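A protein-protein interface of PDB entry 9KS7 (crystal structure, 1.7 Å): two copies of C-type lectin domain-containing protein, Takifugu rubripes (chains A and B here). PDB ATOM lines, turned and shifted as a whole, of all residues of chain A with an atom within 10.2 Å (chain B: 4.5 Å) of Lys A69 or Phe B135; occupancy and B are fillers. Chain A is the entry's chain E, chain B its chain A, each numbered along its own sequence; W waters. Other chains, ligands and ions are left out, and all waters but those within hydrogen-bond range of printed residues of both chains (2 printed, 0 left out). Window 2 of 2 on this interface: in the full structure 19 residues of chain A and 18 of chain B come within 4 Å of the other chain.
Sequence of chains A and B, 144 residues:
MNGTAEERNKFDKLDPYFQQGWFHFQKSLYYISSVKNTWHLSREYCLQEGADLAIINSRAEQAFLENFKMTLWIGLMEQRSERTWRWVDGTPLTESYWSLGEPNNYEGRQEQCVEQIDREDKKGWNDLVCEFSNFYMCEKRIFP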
ATOM      1  N   ILE A  32       2.857 -18.702  37.926  1.00  0.00           N
ATOM      2  CA  ILE A  32       3.628 -18.320  36.748  1.00  0.00           C
ATOM      3  C   ILE A  32       3.248 -16.892  36.393  1.00  0.00           C
ATOM      4  O   ILE A  32       2.057 -16.576  36.273  1.00  0.00           O
ATOM      5  CB  ILE A  32       3.368 -19.284  35.580  1.00  0.00           C
ATOM      6  CG1 ILE A  32       4.016 -20.637  35.882  1.00  0.00           C
ATOM      7  CG2 ILE A  32       3.917 -18.704  34.240  1.00  0.00           C
ATOM      8  CD1 ILE A  32       3.639 -21.733  34.875  1.00  0.00           C
ATOM      9  N   GLN A  62      11.726 -30.865  39.060  1.00  0.00           N
ATOM     10  CA  GLN A  62      12.395 -30.350  37.878  1.00  0.00           C
ATOM     11  C   GLN A  62      11.624 -30.738  36.624  1.00  0.00           C
ATOM     12  O   GLN A  62      11.457 -29.922  35.721  1.00  0.00           O
ATOM     13  CB  GLN A  62      13.829 -30.877  37.807  1.00  0.00           C
ATOM     14  CG  GLN A  62      14.565 -30.452  36.534  1.00  0.00           C
ATOM     15  CD  GLN A  62      14.806 -28.939  36.443  1.00  0.00           C
ATOM     16  OE1 GLN A  62      14.816 -28.231  37.449  1.00  0.00           O
ATOM     17  NE2 GLN A  62      15.034 -28.457  35.226  1.00  0.00           N
ATOM     18  N   ALA A  63      11.136 -31.979  36.557  1.00  0.00           N
ATOM     19  CA  ALA A  63      10.339 -32.399  35.402  1.00  0.00           C
ATOM     20  C   ALA A  63       9.051 -31.580  35.280  1.00  0.00           C
ATOM     21  O   ALA A  63       8.628 -31.221  34.175  1.00  0.00           O
ATOM     22  CB  ALA A  63      10.012 -33.888  35.511  1.00  0.00           C
ATOM     23  N   PHE A  64       8.420 -31.277  36.412  1.00  0.00           N
ATOM     24  CA  PHE A  64       7.235 -30.430  36.416  1.00  0.00           C
ATOM     25  C   PHE A  64       7.577 -29.047  35.858  1.00  0.00           C
ATOM     26  O   PHE A  64       6.896 -28.526  34.954  1.00  0.00           O
ATOM     27  CB  PHE A  64       6.725 -30.415  37.871  1.00  0.00           C
ATOM     28  CG  PHE A  64       5.778 -29.298  38.245  1.00  0.00           C
ATOM     29  CD1 PHE A  64       4.428 -29.373  37.916  1.00  0.00           C
ATOM     30  CD2 PHE A  64       6.217 -28.252  39.060  1.00  0.00           C
ATOM     31  CE1 PHE A  64       3.540 -28.382  38.325  1.00  0.00           C
ATOM     32  CE2 PHE A  64       5.342 -27.243  39.482  1.00  0.00           C
ATOM     33  CZ  PHE A  64       3.995 -27.305  39.106  1.00  0.00           C
ATOM     34  N   LEU A  65       8.687 -28.478  36.328  1.00  0.00           N
ATOM     35  CA  LEU A  65       9.145 -27.180  35.832  1.00  0.00           C
ATOM     36  C   LEU A  65       9.376 -27.226  34.328  1.00  0.00           C
ATOM     37  O   LEU A  65       8.939 -26.335  33.581  1.00  0.00           O
ATOM     38  CB  LEU A  65      10.442 -26.786  36.553  1.00  0.00           C
ATOM     39  CG  LEU A  65      11.175 -25.557  35.987  1.00  0.00           C
ATOM     40  CD1 LEU A  65      10.355 -24.298  36.195  1.00  0.00           C
ATOM     41  CD2 LEU A  65      12.537 -25.425  36.688  1.00  0.00           C
ATOM     42  N   GLU A  66      10.091 -28.257  33.872  1.00  0.00           N
ATOM     43  CA  GLU A  66      10.470 -28.340  32.462  1.00  0.00           C
ATOM     44  C   GLU A  66       9.266 -28.491  31.558  1.00  0.00           C
ATOM     45  O   GLU A  66       9.267 -28.009  30.415  1.00  0.00           O
ATOM     46  CB  GLU A  66      11.435 -29.515  32.240  1.00  0.00           C
ATOM     47  CG  GLU A  66      12.826 -29.103  32.603  1.00  0.00           C
ATOM     48  CD  GLU A  66      13.899 -30.096  32.232  1.00  0.00           C
ATOM     49  OE1 GLU A  66      13.575 -31.136  31.606  1.00  0.00           O
ATOM     50  OE2 GLU A  66      15.087 -29.741  32.445  1.00  0.00           O
ATOM     51  N   ASN A  67       8.229 -29.144  32.051  1.00  0.00           N
ATOM     52  CA  ASN A  67       7.106 -29.470  31.190  1.00  0.00           C
ATOM     53  C   ASN A  67       6.260 -28.247  30.860  1.00  0.00           C
ATOM     54  O   ASN A  67       5.352 -28.342  30.021  1.00  0.00           O
ATOM     55  CB  ASN A  67       6.270 -30.558  31.864  1.00  0.00           C
ATOM     56  CG  ASN A  67       5.257 -31.188  30.910  1.00  0.00           C
ATOM     57  OD1 ASN A  67       5.609 -31.583  29.785  1.00  0.00           O
ATOM     58  ND2 ASN A  67       4.010 -31.280  31.349  1.00  0.00           N
ATOM     59  N   PHE A  68       6.510 -27.107  31.509  1.00  0.00           N
ATOM     60  CA  PHE A  68       5.782 -25.915  31.119  1.00  0.00           C
ATOM     61  C   PHE A  68       6.373 -25.284  29.866  1.00  0.00           C
ATOM     62  O   PHE A  68       5.789 -24.337  29.338  1.00  0.00           O
ATOM     63  CB  PHE A  68       5.749 -24.924  32.285  1.00  0.00           C
ATOM     64  CG  PHE A  68       4.874 -25.414  33.428  1.00  0.00           C
ATOM     65  CD1 PHE A  68       3.515 -25.686  33.204  1.00  0.00           C
ATOM     66  CD2 PHE A  68       5.407 -25.650  34.678  1.00  0.00           C
ATOM     67  CE1 PHE A  68       2.705 -26.171  34.220  1.00  0.00           C
ATOM     68  CE2 PHE A  68       4.592 -26.125  35.713  1.00  0.00           C
ATOM     69  CZ  PHE A  68       3.247 -26.382  35.485  1.00  0.00           C
ATOM     70  N   LYS A  69       7.515 -25.789  29.388  1.00  0.00           N
ATOM     71  CA  LYS A  69       8.049 -25.377  28.092  1.00  0.00           C
ATOM     72  C   LYS A  69       8.269 -23.863  28.050  1.00  0.00           C
ATOM     73  O   LYS A  69       7.943 -23.184  27.078  1.00  0.00           O
ATOM     74  CB  LYS A  69       7.121 -25.858  26.966  1.00  0.00           C
ATOM     75  CG  LYS A  69       6.802 -27.353  27.111  1.00  0.00           C
ATOM     76  CD  LYS A  69       5.942 -27.892  25.945  1.00  0.00           C
ATOM     77  CE  LYS A  69       4.840 -28.848  26.432  1.00  0.00           C
ATOM     78  NZ  LYS A  69       5.370 -29.812  27.424  1.00  0.00           N
ATOM     79  N   MET A  70       8.817 -23.327  29.135  1.00  0.00           N
ATOM     80  CA  MET A  70       8.803 -21.892  29.368  1.00  0.00           C
ATOM     81  C   MET A  70      10.124 -21.491  29.998  1.00  0.00           C
ATOM     82  O   MET A  70      10.556 -22.120  30.966  1.00  0.00           O
ATOM     83  CB  MET A  70       7.667 -21.519  30.340  1.00  0.00           C
ATOM     84  CG  MET A  70       7.390 -20.034  30.442  1.00  0.00           C
ATOM     85  SD  MET A  70       6.011 -19.720  31.589  1.00  0.00           S
ATOM     86  CE  MET A  70       4.584 -20.466  30.735  1.00  0.00           C
ATOM     87  N   THR A  71      10.744 -20.434  29.494  1.00  0.00           N
ATOM     88  CA  THR A  71      11.945 -19.922  30.147  1.00  0.00           C
ATOM     89  C   THR A  71      11.531 -19.120  31.378  1.00  0.00           C
ATOM     90  O   THR A  71      10.734 -18.181  31.273  1.00  0.00           O
ATOM     91  CB  THR A  71      12.738 -19.047  29.176  1.00  0.00           C
ATOM     92  OG1 THR A  71      13.173 -19.856  28.070  1.00  0.00           O
ATOM     93  CG2 THR A  71      13.975 -18.444  29.862  1.00  0.00           C
ATOM     94  N   LEU A  72      12.096 -19.466  32.542  1.00  0.00           N
ATOM     95  CA  LEU A  72      11.602 -18.953  33.818  1.00  0.00           C
ATOM     96  C   LEU A  72      12.756 -18.690  34.775  1.00  0.00           C
ATOM     97  O   LEU A  72      13.609 -19.554  34.952  1.00  0.00           O
ATOM     98  CB  LEU A  72      10.687 -19.971  34.510  1.00  0.00           C
ATOM     99  CG  LEU A  72       9.299 -20.150  33.910  1.00  0.00           C
ATOM    100  CD1 LEU A  72       8.684 -21.491  34.367  1.00  0.00           C
ATOM    101  CD2 LEU A  72       8.432 -18.972  34.379  1.00  0.00           C
ATOM    102  N   GLN A 116      15.530 -21.399  34.232  1.00  0.00           N
ATOM    103  CA  GLN A 116      15.279 -22.621  33.478  1.00  0.00           C
ATOM    104  C   GLN A 116      15.107 -22.202  32.028  1.00  0.00           C
ATOM    105  O   GLN A 116      14.223 -21.397  31.727  1.00  0.00           O
ATOM    106  CB  GLN A 116      14.025 -23.328  33.995  1.00  0.00           C
ATOM    107  CG  GLN A 116      13.462 -24.407  33.050  1.00  0.00           C
ATOM    108  CD  GLN A 116      14.358 -25.635  33.057  1.00  0.00           C
ATOM    109  OE1 GLN A 116      15.165 -25.814  33.981  1.00  0.00           O
ATOM    110  NE2 GLN A 116      14.239 -26.475  32.042  1.00  0.00           N
ATOM    111  N   ILE A 117      15.968 -22.683  31.136  1.00  0.00           N
ATOM    112  CA  ILE A 117      15.880 -22.256  29.743  1.00  0.00           C
ATOM    113  C   ILE A 117      15.101 -23.317  28.984  1.00  0.00           C
ATOM    114  O   ILE A 117      15.237 -24.522  29.246  1.00  0.00           O
ATOM    115  CB  ILE A 117      17.272 -21.998  29.125  1.00  0.00           C
ATOM    116  CG1 ILE A 117      17.141 -21.425  27.711  1.00  0.00           C
ATOM    117  CG2 ILE A 117      18.092 -23.272  29.049  1.00  0.00           C
ATOM    118  CD1 ILE A 117      16.301 -20.168  27.621  1.00  0.00           C
ATOM    119  N   ASP A 118      14.236 -22.876  28.078  1.00  0.00           N
ATOM    120  CA  ASP A 118      13.505 -23.805  27.226  1.00  0.00           C
ATOM    121  C   ASP A 118      13.758 -23.382  25.790  1.00  0.00           C
ATOM    122  O   ASP A 118      13.198 -22.390  25.317  1.00  0.00           O
ATOM    123  CB  ASP A 118      12.015 -23.821  27.511  1.00  0.00           C
ATOM    124  CG  ASP A 118      11.336 -25.027  26.892  1.00  0.00           C
ATOM    125  OD1 ASP A 118      11.636 -26.172  27.314  1.00  0.00           O
ATOM    126  OD2 ASP A 118      10.587 -24.833  25.912  1.00  0.00           O
ATOM    127  N   ARG A 119      14.594 -24.145  25.106  1.00  0.00           N
ATOM    128  CA  ARG A 119      14.888 -23.900  23.711  1.00  0.00           C
ATOM    129  C   ARG A 119      15.072 -25.255  23.049  1.00  0.00           C
ATOM    130  O   ARG A 119      15.299 -26.266  23.719  1.00  0.00           O
ATOM    131  CB  ARG A 119      16.125 -23.007  23.587  1.00  0.00           C
ATOM    132  CG  ARG A 119      15.787 -21.536  23.419  1.00  0.00           C
ATOM    133  CD  ARG A 119      16.998 -20.669  23.723  1.00  0.00           C
ATOM    134  NE  ARG A 119      17.683 -20.215  22.521  1.00  0.00           N
ATOM    135  CZ  ARG A 119      18.966 -20.433  22.272  1.00  0.00           C
ATOM    136  NH1 ARG A 119      19.728 -21.108  23.119  1.00  0.00           N
ATOM    137  NH2 ARG A 119      19.496 -19.969  21.145  1.00  0.00           N
ATOM    138  N   GLU A 120      14.930 -25.290  21.734  1.00  0.00           N
ATOM    139  CA  GLU A 120      15.226 -26.527  21.034  1.00  0.00           C
ATOM    140  C   GLU A 120      16.723 -26.787  21.147  1.00  0.00           C
ATOM    141  O   GLU A 120      17.533 -25.880  20.925  1.00  0.00           O
ATOM    142  CB  GLU A 120      14.785 -26.437  19.576  1.00  0.00           C
ATOM    143  CG  GLU A 120      13.306 -26.740  19.364  1.00  0.00           C
ATOM    144  CD  GLU A 120      12.957 -28.213  19.533  1.00  0.00           C
ATOM    145  OE1 GLU A 120      13.847 -29.072  19.345  1.00  0.00           O
ATOM    146  OE2 GLU A 120      11.781 -28.509  19.839  1.00  0.00           O
ATOM    147  N   LYS A 122      18.373 -27.243  23.883  1.00  0.00           N
ATOM    148  CA  LYS A 122      18.957 -26.632  25.084  1.00  0.00           C
ATOM    149  C   LYS A 122      17.845 -26.500  26.123  1.00  0.00           C
ATOM    150  O   LYS A 122      16.995 -25.610  26.004  1.00  0.00           O
ATOM    151  CB  LYS A 122      19.562 -25.268  24.743  1.00  0.00           C
ATOM    152  CG  LYS A 122      20.538 -24.637  25.755  1.00  0.00           C
ATOM    153  CD  LYS A 122      21.622 -25.572  26.261  1.00  0.00           C
ATOM    154  CE  LYS A 122      22.926 -24.817  26.566  1.00  0.00           C
ATOM    155  NZ  LYS A 122      22.736 -23.643  27.493  1.00  0.00           N
ATOM    156  N   LYS A 123      17.837 -27.383  27.127  1.00  0.00           N
ATOM    157  CA  LYS A 123      16.883 -27.307  28.230  1.00  0.00           C
ATOM    158  C   LYS A 123      17.592 -27.523  29.565  1.00  0.00           C
ATOM    159  O   LYS A 123      18.516 -28.333  29.679  1.00  0.00           O
ATOM    160  CB  LYS A 123      15.755 -28.349  28.098  1.00  0.00           C
ATOM    161  CG  LYS A 123      14.745 -28.119  26.972  1.00  0.00           C
ATOM    162  CD  LYS A 123      15.015 -29.046  25.787  1.00  0.00           C
ATOM    163  CE  LYS A 123      13.839 -29.094  24.809  1.00  0.00           C
ATOM    164  NZ  LYS A 123      13.012 -27.853  24.813  1.00  0.00           N
ATOM    165  N   GLY A 124      17.125 -26.831  30.590  1.00  0.00           N
ATOM    166  CA  GLY A 124      17.689 -26.970  31.920  1.00  0.00           C
ATOM    167  C   GLY A 124      18.153 -25.626  32.435  1.00  0.00           C
ATOM    168  O   GLY A 124      17.854 -24.578  31.862  1.00  0.00           O
ATOM    169  N   PHE A 135       9.995 -14.309  32.300  1.00  0.00           N
ATOM    170  CA  PHE A 135       8.878 -14.726  33.140  1.00  0.00           C
ATOM    171  C   PHE A 135       9.446 -15.411  34.377  1.00  0.00           C
ATOM    172  O   PHE A 135      10.600 -15.830  34.387  1.00  0.00           O
ATOM    173  CB  PHE A 135       7.971 -15.687  32.385  1.00  0.00           C
ATOM    174  CG  PHE A 135       7.270 -15.051  31.205  1.00  0.00           C
ATOM    175  CD1 PHE A 135       6.347 -14.032  31.400  1.00  0.00           C
ATOM    176  CD2 PHE A 135       7.527 -15.496  29.917  1.00  0.00           C
ATOM    177  CE1 PHE A 135       5.686 -13.456  30.312  1.00  0.00           C
ATOM    178  CE2 PHE A 135       6.863 -14.928  28.821  1.00  0.00           C
ATOM    179  CZ  PHE A 135       5.944 -13.907  29.031  1.00  0.00           C
ATOM    180  N   MET A 137       8.595 -17.895  38.162  1.00  0.00           N
ATOM    181  CA  MET A 137       7.723 -18.817  38.879  1.00  0.00           C
ATOM    182  C   MET A 137       7.901 -18.636  40.374  1.00  0.00           C
ATOM    183  O   MET A 137       9.027 -18.764  40.872  1.00  0.00           O
ATOM    184  CB  MET A 137       8.049 -20.268  38.513  1.00  0.00           C
ATOM    185  CG  MET A 137       7.167 -21.281  39.239  1.00  0.00           C
ATOM    186  SD  MET A 137       7.661 -22.949  38.795  1.00  0.00           S
ATOM    187  CE  MET A 137       6.386 -23.361  37.611  1.00  0.00           C
ATOM    188  N   ILE B  32      -0.257 -31.586  31.065  1.00  0.00           N
ATOM    189  CA  ILE B  32       0.194 -30.957  29.823  1.00  0.00           C
ATOM    190  C   ILE B  32       1.104 -31.957  29.110  1.00  0.00           C
ATOM    191  O   ILE B  32       2.032 -32.498  29.719  1.00  0.00           O
ATOM    192  CB  ILE B  32       0.909 -29.624  30.109  1.00  0.00           C
ATOM    193  CG1 ILE B  32      -0.114 -28.558  30.557  1.00  0.00           C
ATOM    194  CG2 ILE B  32       1.663 -29.135  28.871  1.00  0.00           C
ATOM    195  CD1 ILE B  32       0.507 -27.238  30.977  1.00  0.00           C
ATOM    196  N   SER B  33       0.798 -32.261  27.846  1.00  0.00           N
ATOM    197  CA  SER B  33       1.562 -33.299  27.158  1.00  0.00           C
ATOM    198  C   SER B  33       2.975 -32.814  26.872  1.00  0.00           C
ATOM    199  O   SER B  33       3.260 -31.611  26.865  1.00  0.00           O
ATOM    200  CB  SER B  33       0.900 -33.683  25.834  1.00  0.00           C
ATOM    201  OG  SER B  33       0.951 -32.591  24.935  1.00  0.00           O
ATOM    202  N   SER B  34       3.866 -33.783  26.638  1.00  0.00           N
ATOM    203  CA  SER B  34       5.220 -33.483  26.198  1.00  0.00           C
ATOM    204  C   SER B  34       5.432 -33.807  24.724  1.00  0.00           C
ATOM    205  O   SER B  34       6.551 -33.638  24.216  1.00  0.00           O
ATOM    206  CB  SER B  34       6.237 -34.245  27.058  1.00  0.00           C
ATOM    207  OG  SER B  34       5.973 -35.633  27.026  1.00  0.00           O
ATOM    208  N   VAL B  35       4.384 -34.252  24.030  1.00  0.00           N
ATOM    209  CA  VAL B  35       4.390 -34.501  22.594  1.00  0.00           C
ATOM    210  C   VAL B  35       3.173 -33.797  22.009  1.00  0.00           C
ATOM    211  O   VAL B  35       2.194 -33.521  22.706  1.00  0.00           O
ATOM    212  CB  VAL B  35       4.331 -36.008  22.247  1.00  0.00           C
ATOM    213  CG1 VAL B  35       5.609 -36.727  22.756  1.00  0.00           C
ATOM    214  CG2 VAL B  35       3.059 -36.650  22.813  1.00  0.00           C
ATOM    215  N   LYS B  36       3.244 -33.512  20.711  1.00  0.00           N
ATOM    216  CA  LYS B  36       2.086 -32.978  20.007  1.00  0.00           C
ATOM    217  C   LYS B  36       1.315 -34.132  19.376  1.00  0.00           C
ATOM    218  O   LYS B  36       1.872 -35.196  19.087  1.00  0.00           O
ATOM    219  CB  LYS B  36       2.515 -31.996  18.910  1.00  0.00           C
ATOM    220  CG  LYS B  36       3.288 -30.772  19.451  1.00  0.00           C
ATOM    221  CD  LYS B  36       3.383 -29.655  18.415  1.00  0.00           C
ATOM    222  CE  LYS B  36       3.928 -28.356  19.060  1.00  0.00           C
ATOM    223  NZ  LYS B  36       4.119 -27.253  18.048  1.00  0.00           N
ATOM    224  N   MET B  70       0.794 -21.312  25.971  1.00  0.00           N
ATOM    225  CA  MET B  70       1.051 -22.509  25.194  1.00  0.00           C
ATOM    226  C   MET B  70      -0.160 -22.801  24.324  1.00  0.00           C
ATOM    227  O   MET B  70      -1.299 -22.702  24.784  1.00  0.00           O
ATOM    228  CB  MET B  70       1.331 -23.678  26.147  1.00  0.00           C
ATOM    229  CG  MET B  70       1.656 -24.959  25.470  1.00  0.00           C
ATOM    230  SD  MET B  70       1.929 -26.198  26.745  1.00  0.00           S
ATOM    231  CE  MET B  70       3.270 -25.477  27.736  1.00  0.00           C
ATOM    232  N   THR B  71       0.072 -23.138  23.067  1.00  0.00           N
ATOM    233  CA  THR B  71      -1.044 -23.553  22.228  1.00  0.00           C
ATOM    234  C   THR B  71      -1.421 -24.989  22.570  1.00  0.00           C
ATOM    235  O   THR B  71      -0.572 -25.887  22.514  1.00  0.00           O
ATOM    236  CB  THR B  71      -0.653 -23.432  20.765  1.00  0.00           C
ATOM    237  OG1 THR B  71      -0.395 -22.047  20.510  1.00  0.00           O
ATOM    238  CG2 THR B  71      -1.815 -23.921  19.868  1.00  0.00           C
ATOM    239  N   LEU B  72      -2.697 -25.211  22.901  1.00  0.00           N
ATOM    240  CA  LEU B  72      -3.126 -26.500  23.436  1.00  0.00           C
ATOM    241  C   LEU B  72      -4.464 -26.920  22.853  1.00  0.00           C
ATOM    242  O   LEU B  72      -5.398 -26.130  22.845  1.00  0.00           O
ATOM    243  CB  LEU B  72      -3.312 -26.432  24.946  1.00  0.00           C
ATOM    244  CG  LEU B  72      -2.010 -26.372  25.756  1.00  0.00           C
ATOM    245  CD1 LEU B  72      -2.318 -25.726  27.109  1.00  0.00           C
ATOM    246  CD2 LEU B  72      -1.444 -27.779  25.905  1.00  0.00           C
ATOM    247  N   TRP B  73      -4.573 -28.178  22.433  1.00  0.00           N
ATOM    248  CA  TRP B  73      -5.901 -28.730  22.171  1.00  0.00           C
ATOM    249  C   TRP B  73      -6.692 -28.761  23.469  1.00  0.00           C
ATOM    250  O   TRP B  73      -6.151 -29.102  24.522  1.00  0.00           O
ATOM    251  CB  TRP B  73      -5.795 -30.159  21.671  1.00  0.00           C
ATOM    252  CG  TRP B  73      -5.361 -30.350  20.255  1.00  0.00           C
ATOM    253  CD1 TRP B  73      -4.415 -31.265  19.826  1.00  0.00           C
ATOM    254  CD2 TRP B  73      -5.942 -29.788  19.061  1.00  0.00           C
ATOM    255  NE1 TRP B  73      -4.339 -31.246  18.463  1.00  0.00           N
ATOM    256  CE2 TRP B  73      -5.261 -30.363  17.962  1.00  0.00           C
ATOM    257  CE3 TRP B  73      -6.952 -28.847  18.814  1.00  0.00           C
ATOM    258  CZ2 TRP B  73      -5.551 -30.021  16.622  1.00  0.00           C
ATOM    259  CZ3 TRP B  73      -7.246 -28.500  17.469  1.00  0.00           C
ATOM    260  CH2 TRP B  73      -6.549 -29.100  16.397  1.00  0.00           C
ATOM    261  N   ASN B 134      -0.938 -30.464  18.013  1.00  0.00           N
ATOM    262  CA  ASN B 134      -0.676 -29.482  19.058  1.00  0.00           C
ATOM    263  C   ASN B 134      -0.306 -30.257  20.305  1.00  0.00           C
ATOM    264  O   ASN B 134      -0.712 -31.409  20.461  1.00  0.00           O
ATOM    265  CB  ASN B 134      -1.923 -28.666  19.432  1.00  0.00           C
ATOM    266  CG  ASN B 134      -2.176 -27.516  18.519  1.00  0.00           C
ATOM    267  OD1 ASN B 134      -1.269 -26.759  18.168  1.00  0.00           O
ATOM    268  ND2 ASN B 134      -3.463 -27.314  18.194  1.00  0.00           N
ATOM    269  N   PHE B 135       0.392 -29.600  21.230  1.00  0.00           N
ATOM    270  CA  PHE B 135       0.358 -30.120  22.596  1.00  0.00           C
ATOM    271  C   PHE B 135      -1.083 -30.145  23.080  1.00  0.00           C
ATOM    272  O   PHE B 135      -1.957 -29.493  22.503  1.00  0.00           O
ATOM    273  CB  PHE B 135       1.183 -29.234  23.527  1.00  0.00           C
ATOM    274  CG  PHE B 135       2.660 -29.259  23.211  1.00  0.00           C
ATOM    275  CD1 PHE B 135       3.372 -30.442  23.337  1.00  0.00           C
ATOM    276  CD2 PHE B 135       3.309 -28.111  22.773  1.00  0.00           C
ATOM    277  CE1 PHE B 135       4.718 -30.503  23.035  1.00  0.00           C
ATOM    278  CE2 PHE B 135       4.685 -28.156  22.464  1.00  0.00           C
ATOM    279  CZ  PHE B 135       5.375 -29.352  22.603  1.00  0.00           C
ATOM    280  N   TYR B 136      -1.346 -30.918  24.140  1.00  0.00           N
ATOM    281  CA  TYR B 136      -2.721 -31.020  24.595  1.00  0.00           C
ATOM    282  C   TYR B 136      -2.758 -31.001  26.109  1.00  0.00           C
ATOM    283  O   TYR B 136      -1.784 -31.345  26.771  1.00  0.00           O
ATOM    284  CB  TYR B 136      -3.412 -32.297  24.079  1.00  0.00           C
ATOM    285  CG  TYR B 136      -2.617 -33.591  24.245  1.00  0.00           C
ATOM    286  CD1 TYR B 136      -1.659 -33.971  23.308  1.00  0.00           C
ATOM    287  CD2 TYR B 136      -2.852 -34.443  25.335  1.00  0.00           C
ATOM    288  CE1 TYR B 136      -0.943 -35.171  23.435  1.00  0.00           C
ATOM    289  CE2 TYR B 136      -2.131 -35.651  25.470  1.00  0.00           C
ATOM    290  CZ  TYR B 136      -1.184 -36.002  24.515  1.00  0.00           C
ATOM    291  OH  TYR B 136      -0.479 -37.189  24.631  1.00  0.00           O
HETATM  292  O   HOH W   1       1.639 -32.474  33.008  1.00  0.00           O
HETATM  293  O   HOH W   2       4.027 -34.501  29.963  1.00  0.00           O
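O of Ile B32 is in hydrogen-bond range of ND2 of Asn A67. O of Ser B33 is in hydrogen-bond range of NZ of Lys A69, at 2.8 Å.
O of Val B35 sits at hydrogen-bond distance from OG of Ser B33, 2.7 Å away. O of Tyr B136 lies within hydrogen-bond range of N of Ser B33 (2.9 Å). The backbone NH (N) of Trp B73 is in hydrogen-bond range of the backbone carbonyl oxygen (O) of Phe B135, 2.9 Å away. The side-chain amide oxygen of Asn A67 is in hydrogen-bond range of the side-chain amino group of Lys A69 (3.0 Å).
Among the printed residues, merely in contact across the chains: Asn A67 with Ser B33 (3.7 Å), Asn A67 with Ser B34 (3.9 Å), Phe A68 with Met B70 (3.2 Å), Lys A69 with Ser B34 (3.9 Å), Lys A69 with Met B70 (3.9 Å) and Lys A69 with Phe B135 (3.7 Å).
Of the printed residues of chain B, Asn A67 touches Ile B32 (2.8 Å), Ser B33 (3.7 Å) and Ser B34 (3.9 Å). Of the printed residues of chain B, Phe A68 touches Met B70. Printed residues of chain B within 4 Å of Lys A69: Ser B33, Ser B34, Met B70 and Phe B135. Glu A120 touches none of the printed residues of chain B. Of the printed residues of chain A, Ile B32 touches Asn A67 (2.8 Å). Of the printed residues of chain A, Ser B34 touches Asn A67 and Lys A69. No residue of chain A comes within 4 Å of Asn B134. Phe B135 touches one residue of chain A. The nearest printed residue of chain B that does not touch Lys A69 is Ile B32 (4.02 Å). The nearest printed residue of chain B that does not touch Asn A67 is Met B70 (4.2 Å).
Of the 12 printed residues of chain B, 5 touch a printed residue of chain A. Of the 22 printed residues of chain A, 3 touch a printed residue of chain B.
5 positions are printed for both chains. Of the 8 pairs that touch across the chains among the printed residues, none has its exchanged pair printed and touching as well.
Water W2 lies within hydrogen-bond range of the backbone carbonyl oxygen (O) of Ile B32 (2.8 Å), the side-chain amide oxygen (OD1) of Asn A67 (3.3 Å) and the backbone NH (N) of Ser B34 (3.4 Å). Water W1 bridges the backbone NH (N) of Ile B32 (2.9 Å) and the side-chain amide nitrogen (ND2) of Asn A67 (3.1 Å).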
